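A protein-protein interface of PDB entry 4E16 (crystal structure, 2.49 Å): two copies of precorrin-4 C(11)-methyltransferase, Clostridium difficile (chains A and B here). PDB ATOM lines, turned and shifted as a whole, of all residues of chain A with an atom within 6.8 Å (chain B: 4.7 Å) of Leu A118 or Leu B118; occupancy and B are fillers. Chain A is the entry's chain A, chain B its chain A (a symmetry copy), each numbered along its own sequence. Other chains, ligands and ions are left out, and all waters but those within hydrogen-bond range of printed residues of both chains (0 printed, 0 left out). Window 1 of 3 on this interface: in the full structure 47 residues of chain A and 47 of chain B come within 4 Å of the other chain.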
ATOM      1  N   PRO A  14      -0.079  -9.018 -27.025  1.00  0.00           N
ATOM      2  CA  PRO A  14       1.275  -9.464 -27.412  1.00  0.00           C
ATOM      3  C   PRO A  14       2.318  -8.369 -27.589  1.00  0.00           C
ATOM      4  O   PRO A  14       3.465  -8.675 -27.984  1.00  0.00           O
ATOM      5  CB  PRO A  14       1.035 -10.124 -28.777  1.00  0.00           C
ATOM      6  CG  PRO A  14      -0.191  -9.421 -29.334  1.00  0.00           C
ATOM      7  CD  PRO A  14      -1.063  -9.110 -28.142  1.00  0.00           C
ATOM      8  N   ASP A  87      -1.436 -13.974 -22.784  1.00  0.00           N
ATOM      9  CA  ASP A  87      -2.399 -14.595 -21.889  1.00  0.00           C
ATOM     10  C   ASP A  87      -1.700 -15.603 -20.984  1.00  0.00           C
ATOM     11  O   ASP A  87      -0.800 -16.354 -21.404  1.00  0.00           O
ATOM     12  CB  ASP A  87      -3.584 -15.246 -22.632  1.00  0.00           C
ATOM     13  CG  ASP A  87      -4.758 -15.617 -21.684  1.00  0.00           C
ATOM     14  OD1 ASP A  87      -4.837 -15.069 -20.559  1.00  0.00           O
ATOM     15  OD2 ASP A  87      -5.610 -16.458 -22.056  1.00  0.00           O
ATOM     16  N   PHE A  88      -2.178 -15.586 -19.742  1.00  0.00           N
ATOM     17  CA  PHE A  88      -1.655 -16.323 -18.597  1.00  0.00           C
ATOM     18  C   PHE A  88      -2.124 -17.784 -18.476  1.00  0.00           C
ATOM     19  O   PHE A  88      -1.639 -18.531 -17.616  1.00  0.00           O
ATOM     20  CB  PHE A  88      -1.981 -15.554 -17.302  1.00  0.00           C
ATOM     21  CG  PHE A  88      -3.285 -14.804 -17.349  1.00  0.00           C
ATOM     22  CD1 PHE A  88      -3.292 -13.411 -17.464  1.00  0.00           C
ATOM     23  CD2 PHE A  88      -4.503 -15.488 -17.291  1.00  0.00           C
ATOM     24  CE1 PHE A  88      -4.494 -12.717 -17.517  1.00  0.00           C
ATOM     25  CE2 PHE A  88      -5.698 -14.796 -17.357  1.00  0.00           C
ATOM     26  CZ  PHE A  88      -5.696 -13.410 -17.464  1.00  0.00           C
ATOM     27  N   SER A  89      -3.053 -18.179 -19.338  1.00  0.00           N
ATOM     28  CA  SER A  89      -3.382 -19.586 -19.520  1.00  0.00           C
ATOM     29  C   SER A  89      -2.298 -20.338 -20.345  1.00  0.00           C
ATOM     30  O   SER A  89      -2.211 -21.549 -20.280  1.00  0.00           O
ATOM     31  CB  SER A  89      -4.727 -19.674 -20.185  1.00  0.00           C
ATOM     32  OG  SER A  89      -4.703 -18.812 -21.292  1.00  0.00           O
ATOM     33  N   ILE A  90      -1.457 -19.617 -21.087  1.00  0.00           N
ATOM     34  CA  ILE A  90      -0.341 -20.237 -21.794  1.00  0.00           C
ATOM     35  C   ILE A  90       0.929 -19.533 -21.358  1.00  0.00           C
ATOM     36  O   ILE A  90       1.215 -18.426 -21.843  1.00  0.00           O
ATOM     37  CB  ILE A  90      -0.511 -20.111 -23.330  1.00  0.00           C
ATOM     38  CG1 ILE A  90      -1.729 -20.902 -23.802  1.00  0.00           C
ATOM     39  CG2 ILE A  90       0.720 -20.595 -24.097  1.00  0.00           C
ATOM     40  CD1 ILE A  90      -2.139 -20.471 -25.190  1.00  0.00           C
ATOM     41  N   PRO A 112      -8.874 -12.246 -20.016  1.00  0.00           N
ATOM     42  CA  PRO A 112      -7.929 -12.788 -20.996  1.00  0.00           C
ATOM     43  C   PRO A 112      -7.413 -11.767 -21.972  1.00  0.00           C
ATOM     44  O   PRO A 112      -8.058 -10.740 -22.163  1.00  0.00           O
ATOM     45  CB  PRO A 112      -8.776 -13.798 -21.773  1.00  0.00           C
ATOM     46  CG  PRO A 112     -10.170 -13.317 -21.595  1.00  0.00           C
ATOM     47  CD  PRO A 112     -10.219 -12.807 -20.186  1.00  0.00           C
ATOM     48  N   GLY A 113      -6.265 -12.068 -22.588  1.00  0.00           N
ATOM     49  CA  GLY A 113      -5.707 -11.276 -23.693  1.00  0.00           C
ATOM     50  C   GLY A 113      -5.315 -12.066 -24.925  1.00  0.00           C
ATOM     51  O   GLY A 113      -5.400 -13.307 -24.947  1.00  0.00           O
ATOM     52  N   VAL A 114      -4.924 -11.338 -25.968  1.00  0.00           N
ATOM     53  CA  VAL A 114      -4.419 -11.900 -27.230  1.00  0.00           C
ATOM     54  C   VAL A 114      -3.013 -12.509 -27.093  1.00  0.00           C
ATOM     55  O   VAL A 114      -2.018 -11.774 -26.869  1.00  0.00           O
ATOM     56  CB  VAL A 114      -4.385 -10.792 -28.289  1.00  0.00           C
ATOM     57  CG1 VAL A 114      -3.889 -11.274 -29.647  1.00  0.00           C
ATOM     58  CG2 VAL A 114      -5.757 -10.181 -28.425  1.00  0.00           C
ATOM     59  N   SER A 115      -2.930 -13.838 -27.242  1.00  0.00           N
ATOM     60  CA  SER A 115      -1.646 -14.531 -27.206  1.00  0.00           C
ATOM     61  C   SER A 115      -0.709 -14.064 -28.325  1.00  0.00           C
ATOM     62  O   SER A 115      -1.145 -13.628 -29.395  1.00  0.00           O
ATOM     63  CB  SER A 115      -1.873 -16.026 -27.309  1.00  0.00           C
ATOM     64  OG  SER A 115      -1.515 -16.670 -26.106  1.00  0.00           O
ATOM     65  N   SER A 116       0.582 -14.154 -28.101  1.00  0.00           N
ATOM     66  CA  SER A 116       1.535 -13.629 -29.111  1.00  0.00           C
ATOM     67  C   SER A 116       1.518 -14.504 -30.336  1.00  0.00           C
ATOM     68  O   SER A 116       1.767 -14.031 -31.475  1.00  0.00           O
ATOM     69  CB  SER A 116       2.941 -13.595 -28.564  1.00  0.00           C
ATOM     70  OG  SER A 116       3.078 -14.696 -27.671  1.00  0.00           O
ATOM     71  N   PHE A 117       1.227 -15.788 -30.139  1.00  0.00           N
ATOM     72  CA  PHE A 117       1.119 -16.599 -31.321  1.00  0.00           C
ATOM     73  C   PHE A 117      -0.067 -16.208 -32.204  1.00  0.00           C
ATOM     74  O   PHE A 117       0.005 -16.377 -33.410  1.00  0.00           O
ATOM     75  CB  PHE A 117       1.232 -18.088 -31.026  1.00  0.00           C
ATOM     76  CG  PHE A 117       0.111 -18.632 -30.261  1.00  0.00           C
ATOM     77  CD1 PHE A 117      -1.044 -19.056 -30.912  1.00  0.00           C
ATOM     78  CD2 PHE A 117       0.212 -18.769 -28.882  1.00  0.00           C
ATOM     79  CE1 PHE A 117      -2.096 -19.603 -30.198  1.00  0.00           C
ATOM     80  CE2 PHE A 117      -0.844 -19.301 -28.154  1.00  0.00           C
ATOM     81  CZ  PHE A 117      -2.011 -19.694 -28.806  1.00  0.00           C
ATOM     82  N   LEU A 118      -1.113 -15.605 -31.624  1.00  0.00           N
ATOM     83  CA  LEU A 118      -2.200 -15.008 -32.449  1.00  0.00           C
ATOM     84  C   LEU A 118      -1.719 -13.752 -33.145  1.00  0.00           C
ATOM     85  O   LEU A 118      -1.999 -13.544 -34.339  1.00  0.00           O
ATOM     86  CB  LEU A 118      -3.463 -14.732 -31.629  1.00  0.00           C
ATOM     87  CG  LEU A 118      -3.989 -15.982 -30.861  1.00  0.00           C
ATOM     88  CD1 LEU A 118      -5.172 -15.679 -29.927  1.00  0.00           C
ATOM     89  CD2 LEU A 118      -4.325 -17.141 -31.810  1.00  0.00           C
ATOM     90  N   GLY A 119      -0.980 -12.927 -32.391  1.00  0.00           N
ATOM     91  CA  GLY A 119      -0.350 -11.704 -32.914  1.00  0.00           C
ATOM     92  C   GLY A 119       0.555 -12.014 -34.079  1.00  0.00           C
ATOM     93  O   GLY A 119       0.490 -11.335 -35.122  1.00  0.00           O
ATOM     94  N   ALA A 120       1.369 -13.068 -33.912  1.00  0.00           N
ATOM     95  CA  ALA A 120       2.311 -13.557 -34.958  1.00  0.00           C
ATOM     96  C   ALA A 120       1.600 -13.965 -36.217  1.00  0.00           C
ATOM     97  O   ALA A 120       1.998 -13.553 -37.323  1.00  0.00           O
ATOM     98  CB  ALA A 120       3.134 -14.726 -34.449  1.00  0.00           C
ATOM     99  N   ALA A 121       0.540 -14.765 -36.075  1.00  0.00           N
ATOM    100  CA  ALA A 121      -0.230 -15.094 -37.276  1.00  0.00           C
ATOM    101  C   ALA A 121      -0.750 -13.851 -38.060  1.00  0.00           C
ATOM    102  O   ALA A 121      -0.540 -13.754 -39.272  1.00  0.00           O
ATOM    103  CB  ALA A 121      -1.335 -16.073 -36.969  1.00  0.00           C
ATOM    104  N   SER A 122      -1.386 -12.893 -37.377  1.00  0.00           N
ATOM    105  CA  SER A 122      -2.022 -11.758 -38.072  1.00  0.00           C
ATOM    106  C   SER A 122      -0.949 -10.977 -38.761  1.00  0.00           C
ATOM    107  O   SER A 122      -1.041 -10.614 -39.956  1.00  0.00           O
ATOM    108  CB  SER A 122      -2.711 -10.838 -37.077  1.00  0.00           C
ATOM    109  OG  SER A 122      -3.470 -11.598 -36.158  1.00  0.00           O
ATOM    110  N   SER A 123       0.089 -10.757 -37.967  1.00  0.00           N
ATOM    111  CA  SER A 123       1.293 -10.083 -38.383  1.00  0.00           C
ATOM    112  C   SER A 123       1.846 -10.736 -39.633  1.00  0.00           C
ATOM    113  O   SER A 123       2.150 -10.062 -40.599  1.00  0.00           O
ATOM    114  CB  SER A 123       2.295 -10.113 -37.233  1.00  0.00           C
ATOM    115  OG  SER A 123       3.529  -9.635 -37.683  1.00  0.00           O
ATOM    116  N   LEU A 124       1.944 -12.060 -39.638  1.00  0.00           N
ATOM    117  CA  LEU A 124       2.320 -12.765 -40.859  1.00  0.00           C
ATOM    118  C   LEU A 124       1.181 -12.925 -41.894  1.00  0.00           C
ATOM    119  O   LEU A 124       1.416 -13.464 -42.977  1.00  0.00           O
ATOM    120  CB  LEU A 124       2.849 -14.150 -40.499  1.00  0.00           C
ATOM    121  CG  LEU A 124       4.341 -14.366 -40.298  1.00  0.00           C
ATOM    122  CD1 LEU A 124       4.503 -15.771 -39.775  1.00  0.00           C
ATOM    123  CD2 LEU A 124       5.098 -14.211 -41.611  1.00  0.00           C
ATOM    124  N   VAL A 126      -1.508 -15.126 -41.857  1.00  0.00           N
ATOM    125  CA  VAL A 126      -1.357 -16.567 -42.099  1.00  0.00           C
ATOM    126  C   VAL A 126      -2.330 -17.229 -41.140  1.00  0.00           C
ATOM    127  O   VAL A 126      -2.756 -16.602 -40.130  1.00  0.00           O
ATOM    128  CB  VAL A 126       0.132 -17.000 -41.894  1.00  0.00           C
ATOM    129  CG1 VAL A 126       0.409 -17.533 -40.486  1.00  0.00           C
ATOM    130  CG2 VAL A 126       0.623 -17.946 -42.974  1.00  0.00           C
ATOM    131  N   TYR A 128      -3.193 -20.877 -39.082  1.00  0.00           N
ATOM    132  CA  TYR A 128      -2.714 -22.161 -38.581  1.00  0.00           C
ATOM    133  C   TYR A 128      -3.463 -23.357 -39.163  1.00  0.00           C
ATOM    134  O   TYR A 128      -2.857 -24.404 -39.499  1.00  0.00           O
ATOM    135  CB  TYR A 128      -2.751 -22.202 -37.031  1.00  0.00           C
ATOM    136  CG  TYR A 128      -1.744 -21.292 -36.369  1.00  0.00           C
ATOM    137  CD1 TYR A 128      -0.336 -21.625 -36.352  1.00  0.00           C
ATOM    138  CD2 TYR A 128      -2.153 -20.070 -35.791  1.00  0.00           C
ATOM    139  CE1 TYR A 128       0.600 -20.767 -35.764  1.00  0.00           C
ATOM    140  CE2 TYR A 128      -1.219 -19.201 -35.189  1.00  0.00           C
ATOM    141  CZ  TYR A 128       0.143 -19.542 -35.172  1.00  0.00           C
ATOM    142  OH  TYR A 128       1.033 -18.669 -34.589  1.00  0.00           O
ATOM    143  N   THR A 198       4.333  -8.046 -33.153  1.00  0.00           N
ATOM    144  CA  THR A 198       3.453  -6.829 -33.041  1.00  0.00           C
ATOM    145  C   THR A 198       4.009  -5.633 -32.278  1.00  0.00           C
ATOM    146  O   THR A 198       3.323  -4.619 -32.149  1.00  0.00           O
ATOM    147  CB  THR A 198       2.085  -7.088 -32.379  1.00  0.00           C
ATOM    148  OG1 THR A 198       2.265  -7.111 -30.949  1.00  0.00           O
ATOM    149  CG2 THR A 198       1.459  -8.366 -32.894  1.00  0.00           C
ATOM    150  N   LEU A 226       9.169 -16.686 -31.247  1.00  0.00           N
ATOM    151  CA  LEU A 226       8.243 -17.738 -31.679  1.00  0.00           C
ATOM    152  C   LEU A 226       8.779 -18.370 -32.937  1.00  0.00           C
ATOM    153  O   LEU A 226       9.082 -17.674 -33.944  1.00  0.00           O
ATOM    154  CB  LEU A 226       6.899 -17.195 -32.083  1.00  0.00           C
ATOM    155  CG  LEU A 226       6.130 -16.614 -30.935  1.00  0.00           C
ATOM    156  CD1 LEU A 226       4.685 -16.524 -31.376  1.00  0.00           C
ATOM    157  CD2 LEU A 226       6.293 -17.512 -29.712  1.00  0.00           C
ATOM    158  N   ASP B  87     -10.411 -15.589 -33.267  1.00  0.00           N
ATOM    159  CA  ASP B  87      -9.351 -15.250 -34.202  1.00  0.00           C
ATOM    160  C   ASP B  87      -9.369 -16.208 -35.387  1.00  0.00           C
ATOM    161  O   ASP B  87      -9.588 -17.427 -35.246  1.00  0.00           O
ATOM    162  CB  ASP B  87      -7.955 -15.207 -33.545  1.00  0.00           C
ATOM    163  CG  ASP B  87      -6.885 -14.538 -34.451  1.00  0.00           C
ATOM    164  OD1 ASP B  87      -7.252 -13.796 -35.392  1.00  0.00           O
ATOM    165  OD2 ASP B  87      -5.670 -14.748 -34.228  1.00  0.00           O
ATOM    166  N   SER B  89      -6.879 -16.921 -37.501  1.00  0.00           N
ATOM    167  CA  SER B  89      -5.749 -17.828 -37.647  1.00  0.00           C
ATOM    168  C   SER B  89      -6.077 -19.259 -37.132  1.00  0.00           C
ATOM    169  O   SER B  89      -5.417 -20.209 -37.505  1.00  0.00           O
ATOM    170  CB  SER B  89      -4.575 -17.243 -36.911  1.00  0.00           C
ATOM    171  OG  SER B  89      -5.022 -16.884 -35.630  1.00  0.00           O
ATOM    172  N   ILE B  90      -7.116 -19.410 -36.310  1.00  0.00           N
ATOM    173  CA  ILE B  90      -7.560 -20.732 -35.879  1.00  0.00           C
ATOM    174  C   ILE B  90      -9.028 -20.864 -36.233  1.00  0.00           C
ATOM    175  O   ILE B  90      -9.884 -20.323 -35.514  1.00  0.00           O
ATOM    176  CB  ILE B  90      -7.370 -20.917 -34.351  1.00  0.00           C
ATOM    177  CG1 ILE B  90      -5.886 -20.892 -33.988  1.00  0.00           C
ATOM    178  CG2 ILE B  90      -7.981 -22.221 -33.838  1.00  0.00           C
ATOM    179  CD1 ILE B  90      -5.704 -20.664 -32.507  1.00  0.00           C
ATOM    180  N   PRO B 112      -5.823  -9.079 -34.864  1.00  0.00           N
ATOM    181  CA  PRO B 112      -6.157 -10.307 -34.135  1.00  0.00           C
ATOM    182  C   PRO B 112      -7.100 -10.093 -32.984  1.00  0.00           C
ATOM    183  O   PRO B 112      -7.197  -8.975 -32.488  1.00  0.00           O
ATOM    184  CB  PRO B 112      -4.807 -10.748 -33.564  1.00  0.00           C
ATOM    185  CG  PRO B 112      -4.013  -9.495 -33.496  1.00  0.00           C
ATOM    186  CD  PRO B 112      -4.406  -8.729 -34.724  1.00  0.00           C
ATOM    187  N   GLY B 113      -7.771 -11.171 -32.564  1.00  0.00           N
ATOM    188  CA  GLY B 113      -8.598 -11.188 -31.349  1.00  0.00           C
ATOM    189  C   GLY B 113      -8.321 -12.329 -30.391  1.00  0.00           C
ATOM    190  O   GLY B 113      -7.498 -13.219 -30.672  1.00  0.00           O
ATOM    191  N   VAL B 114      -8.982 -12.277 -29.237  1.00  0.00           N
ATOM    192  CA  VAL B 114      -8.931 -13.323 -28.204  1.00  0.00           C
ATOM    193  C   VAL B 114      -9.683 -14.601 -28.609  1.00  0.00           C
ATOM    194  O   VAL B 114     -10.934 -14.594 -28.728  1.00  0.00           O
ATOM    195  CB  VAL B 114      -9.538 -12.772 -26.909  1.00  0.00           C
ATOM    196  CG1 VAL B 114      -9.520 -13.775 -25.762  1.00  0.00           C
ATOM    197  CG2 VAL B 114      -8.814 -11.511 -26.507  1.00  0.00           C
ATOM    198  N   SER B 115      -8.929 -15.692 -28.804  1.00  0.00           N
ATOM    199  CA  SER B 115      -9.526 -16.985 -29.123  1.00  0.00           C
ATOM    200  C   SER B 115     -10.453 -17.481 -28.007  1.00  0.00           C
ATOM    201  O   SER B 115     -10.281 -17.154 -26.830  1.00  0.00           O
ATOM    202  CB  SER B 115      -8.429 -18.001 -29.377  1.00  0.00           C
ATOM    203  OG  SER B 115      -8.426 -18.404 -30.729  1.00  0.00           O
ATOM    204  N   SER B 116     -11.437 -18.276 -28.358  1.00  0.00           N
ATOM    205  CA  SER B 116     -12.422 -18.711 -27.335  1.00  0.00           C
ATOM    206  C   SER B 116     -11.771 -19.666 -26.370  1.00  0.00           C
ATOM    207  O   SER B 116     -12.157 -19.744 -25.175  1.00  0.00           O
ATOM    208  CB  SER B 116     -13.600 -19.402 -27.975  1.00  0.00           C
ATOM    209  OG  SER B 116     -13.117 -20.093 -29.123  1.00  0.00           O
ATOM    210  N   PHE B 117     -10.779 -20.409 -26.855  1.00  0.00           N
ATOM    211  CA  PHE B 117     -10.099 -21.250 -25.908  1.00  0.00           C
ATOM    212  C   PHE B 117      -9.323 -20.456 -24.857  1.00  0.00           C
ATOM    213  O   PHE B 117      -9.174 -20.928 -23.742  1.00  0.00           O
ATOM    214  CB  PHE B 117      -9.311 -22.369 -26.574  1.00  0.00           C
ATOM    215  CG  PHE B 117      -8.160 -21.908 -27.351  1.00  0.00           C
ATOM    216  CD1 PHE B 117      -6.934 -21.689 -26.728  1.00  0.00           C
ATOM    217  CD2 PHE B 117      -8.276 -21.728 -28.724  1.00  0.00           C
ATOM    218  CE1 PHE B 117      -5.833 -21.285 -27.463  1.00  0.00           C
ATOM    219  CE2 PHE B 117      -7.182 -21.307 -29.467  1.00  0.00           C
ATOM    220  CZ  PHE B 117      -5.966 -21.058 -28.836  1.00  0.00           C
ATOM    221  N   LEU B 118      -8.914 -19.221 -25.175  1.00  0.00           N
ATOM    222  CA  LEU B 118      -8.346 -18.317 -24.136  1.00  0.00           C
ATOM    223  C   LEU B 118      -9.428 -17.834 -23.194  1.00  0.00           C
ATOM    224  O   LEU B 118      -9.230 -17.805 -21.965  1.00  0.00           O
ATOM    225  CB  LEU B 118      -7.587 -17.136 -24.750  1.00  0.00           C
ATOM    226  CG  LEU B 118      -6.478 -17.569 -25.757  1.00  0.00           C
ATOM    227  CD1 LEU B 118      -5.809 -16.389 -26.480  1.00  0.00           C
ATOM    228  CD2 LEU B 118      -5.428 -18.476 -25.102  1.00  0.00           C
ATOM    229  N   GLY B 119     -10.578 -17.473 -23.779  1.00  0.00           N
ATOM    230  CA  GLY B 119     -11.773 -17.063 -23.024  1.00  0.00           C
ATOM    231  C   GLY B 119     -12.199 -18.136 -22.056  1.00  0.00           C
ATOM    232  O   GLY B 119     -12.470 -17.845 -20.875  1.00  0.00           O
ATOM    233  N   ALA B 120     -12.217 -19.384 -22.550  1.00  0.00           N
ATOM    234  CA  ALA B 120     -12.574 -20.586 -21.744  1.00  0.00           C
ATOM    235  C   ALA B 120     -11.656 -20.777 -20.570  1.00  0.00           C
ATOM    236  O   ALA B 120     -12.125 -20.984 -19.435  1.00  0.00           O
ATOM    237  CB  ALA B 120     -12.558 -21.841 -22.598  1.00  0.00           C
ATOM    238  N   ALA B 121     -10.345 -20.701 -20.815  1.00  0.00           N
ATOM    239  CA  ALA B 121      -9.433 -20.782 -19.673  1.00  0.00           C
ATOM    240  C   ALA B 121      -9.710 -19.723 -18.561  1.00  0.00           C
ATOM    241  O   ALA B 121      -9.830 -20.080 -17.387  1.00  0.00           O
ATOM    242  CB  ALA B 121      -7.992 -20.772 -20.117  1.00  0.00           C
ATOM    243  N   SER B 122      -9.847 -18.445 -18.926  1.00  0.00           N
ATOM    244  CA  SER B 122      -9.975 -17.375 -17.918  1.00  0.00           C
ATOM    245  C   SER B 122     -11.237 -17.609 -17.151  1.00  0.00           C
ATOM    246  O   SER B 122     -11.281 -17.577 -15.899  1.00  0.00           O
ATOM    247  CB  SER B 122     -10.075 -16.014 -18.588  1.00  0.00           C
ATOM    248  OG  SER B 122      -9.093 -15.898 -19.599  1.00  0.00           O
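The side-chain carboxylate (OD2) of Asp A87 sits at hydrogen-bond distance from the side-chain hydroxyl (OG) of Ser A89 (2.6 Å).
The backbone carbonyl oxygen (O) of Phe A117 sits at hydrogen-bond distance from the side-chain hydroxyl (OH) of Tyr A128, 2.8 Å away.
The side-chain hydroxyl of Ser A122 is in hydrogen-bond range of the backbone carbonyl oxygen of Leu A118 (3.0 Å).
The backbone carbonyl oxygen (O) of Ala A121 is in hydrogen-bond range of the backbone NH (N) of Val A126 (3.1 Å).
The side-chain carboxylate (OD2) of Asp B87 sits at hydrogen-bond distance from the side-chain hydroxyl (OG) of Ser B89 (2.6 Å).
The backbone carbonyl oxygen (O) of Leu B118 lies within hydrogen-bond range of the side-chain hydroxyl (OG) of Ser B122 (3.0 Å).
Leu A118 touches just these residues of chain B: Asp B87 (3.4 Å), Ser B89 (3.9 Å), Ile B90 (3.8 Å), Gly B113 (3.5 Å), Ser B115 (3.9 Å) and Leu B118 (3.6 Å).
Leu B118 touches just these residues of chain A: Asp A87 (3.4 Å), Ser A89 (3.9 Å), Ile A90 (3.8 Å), Gly A113 (3.5 Å), Ser A115 (3.9 Å) and Leu A118 (3.6 Å).
Printed residues of chain B within 4 Å of Ile A90: Leu B118.
Printed residues of chain A within 4 Å of Ile B90: Leu A118 (3.8 Å).
The nearest residue of chain B that does not touch Leu A118 is Pro B112 (4.04 Å).
Among the printed residues, merely in contact across the chains: Asp A87 with Leu B118 (3.4 Å), Ser A89 with Leu B118 (3.9 Å), Ser A89 with Ala B121 (3.4 Å), Ile A90 with Leu B118 (3.8 Å), Pro A112 with Ser B122 (3.0 Å), Gly A113 with Val B114 (3.9 Å), Gly A113 with Leu B118 (3.5 Å), Val A114 with Gly B113 (3.9 Å), Val A114 with Val B114 (3.8 Å), Ser A115 with Leu B118 (3.9 Å), Leu A118 with Asp B87 (3.4 Å), Leu A118 with Ser B89 (3.9 Å), Leu A118 with Ile B90 (3.8 Å), Leu A118 with Gly B113 (3.5 Å), Leu A118 with Ser B115 (3.9 Å), Leu A118 with Leu B118 (3.6 Å), Ala A121 with Ser B89 (3.4 Å), Ser A122 with Pro B112 (3.0 Å) and Val A126 with Ser B89 (3.8 Å).
Along chain B the printed residues that touch a printed residue of chain A span positions 87 to 122.
Of the 22 printed residues of chain A, 12 touch a printed residue of chain B.
Among the printed residues, 20 pairs touch across the chains.
Among the printed residues, no Asp or Glu carboxylate lies within 4 Å of a Lys or Arg side-chain nitrogen of the other chain.
Pro A112 touches Ser B122, and with the chains exchanged Ser A122 touches Pro B112.
Gly A113 touches Val B114, and with the chains exchanged Val A114 touches Gly B113.
Gly A113 touches Leu B118, and with the chains exchanged Leu A118 touches Gly B113.
Val A114 touches its own counterpart, Val B114.
14 positions are printed for both chains.
The backbone carbonyl oxygen (O) of Ser B89 lies within hydrogen-bond range of the backbone NH (N) of Tyr A128 (2.8 Å).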
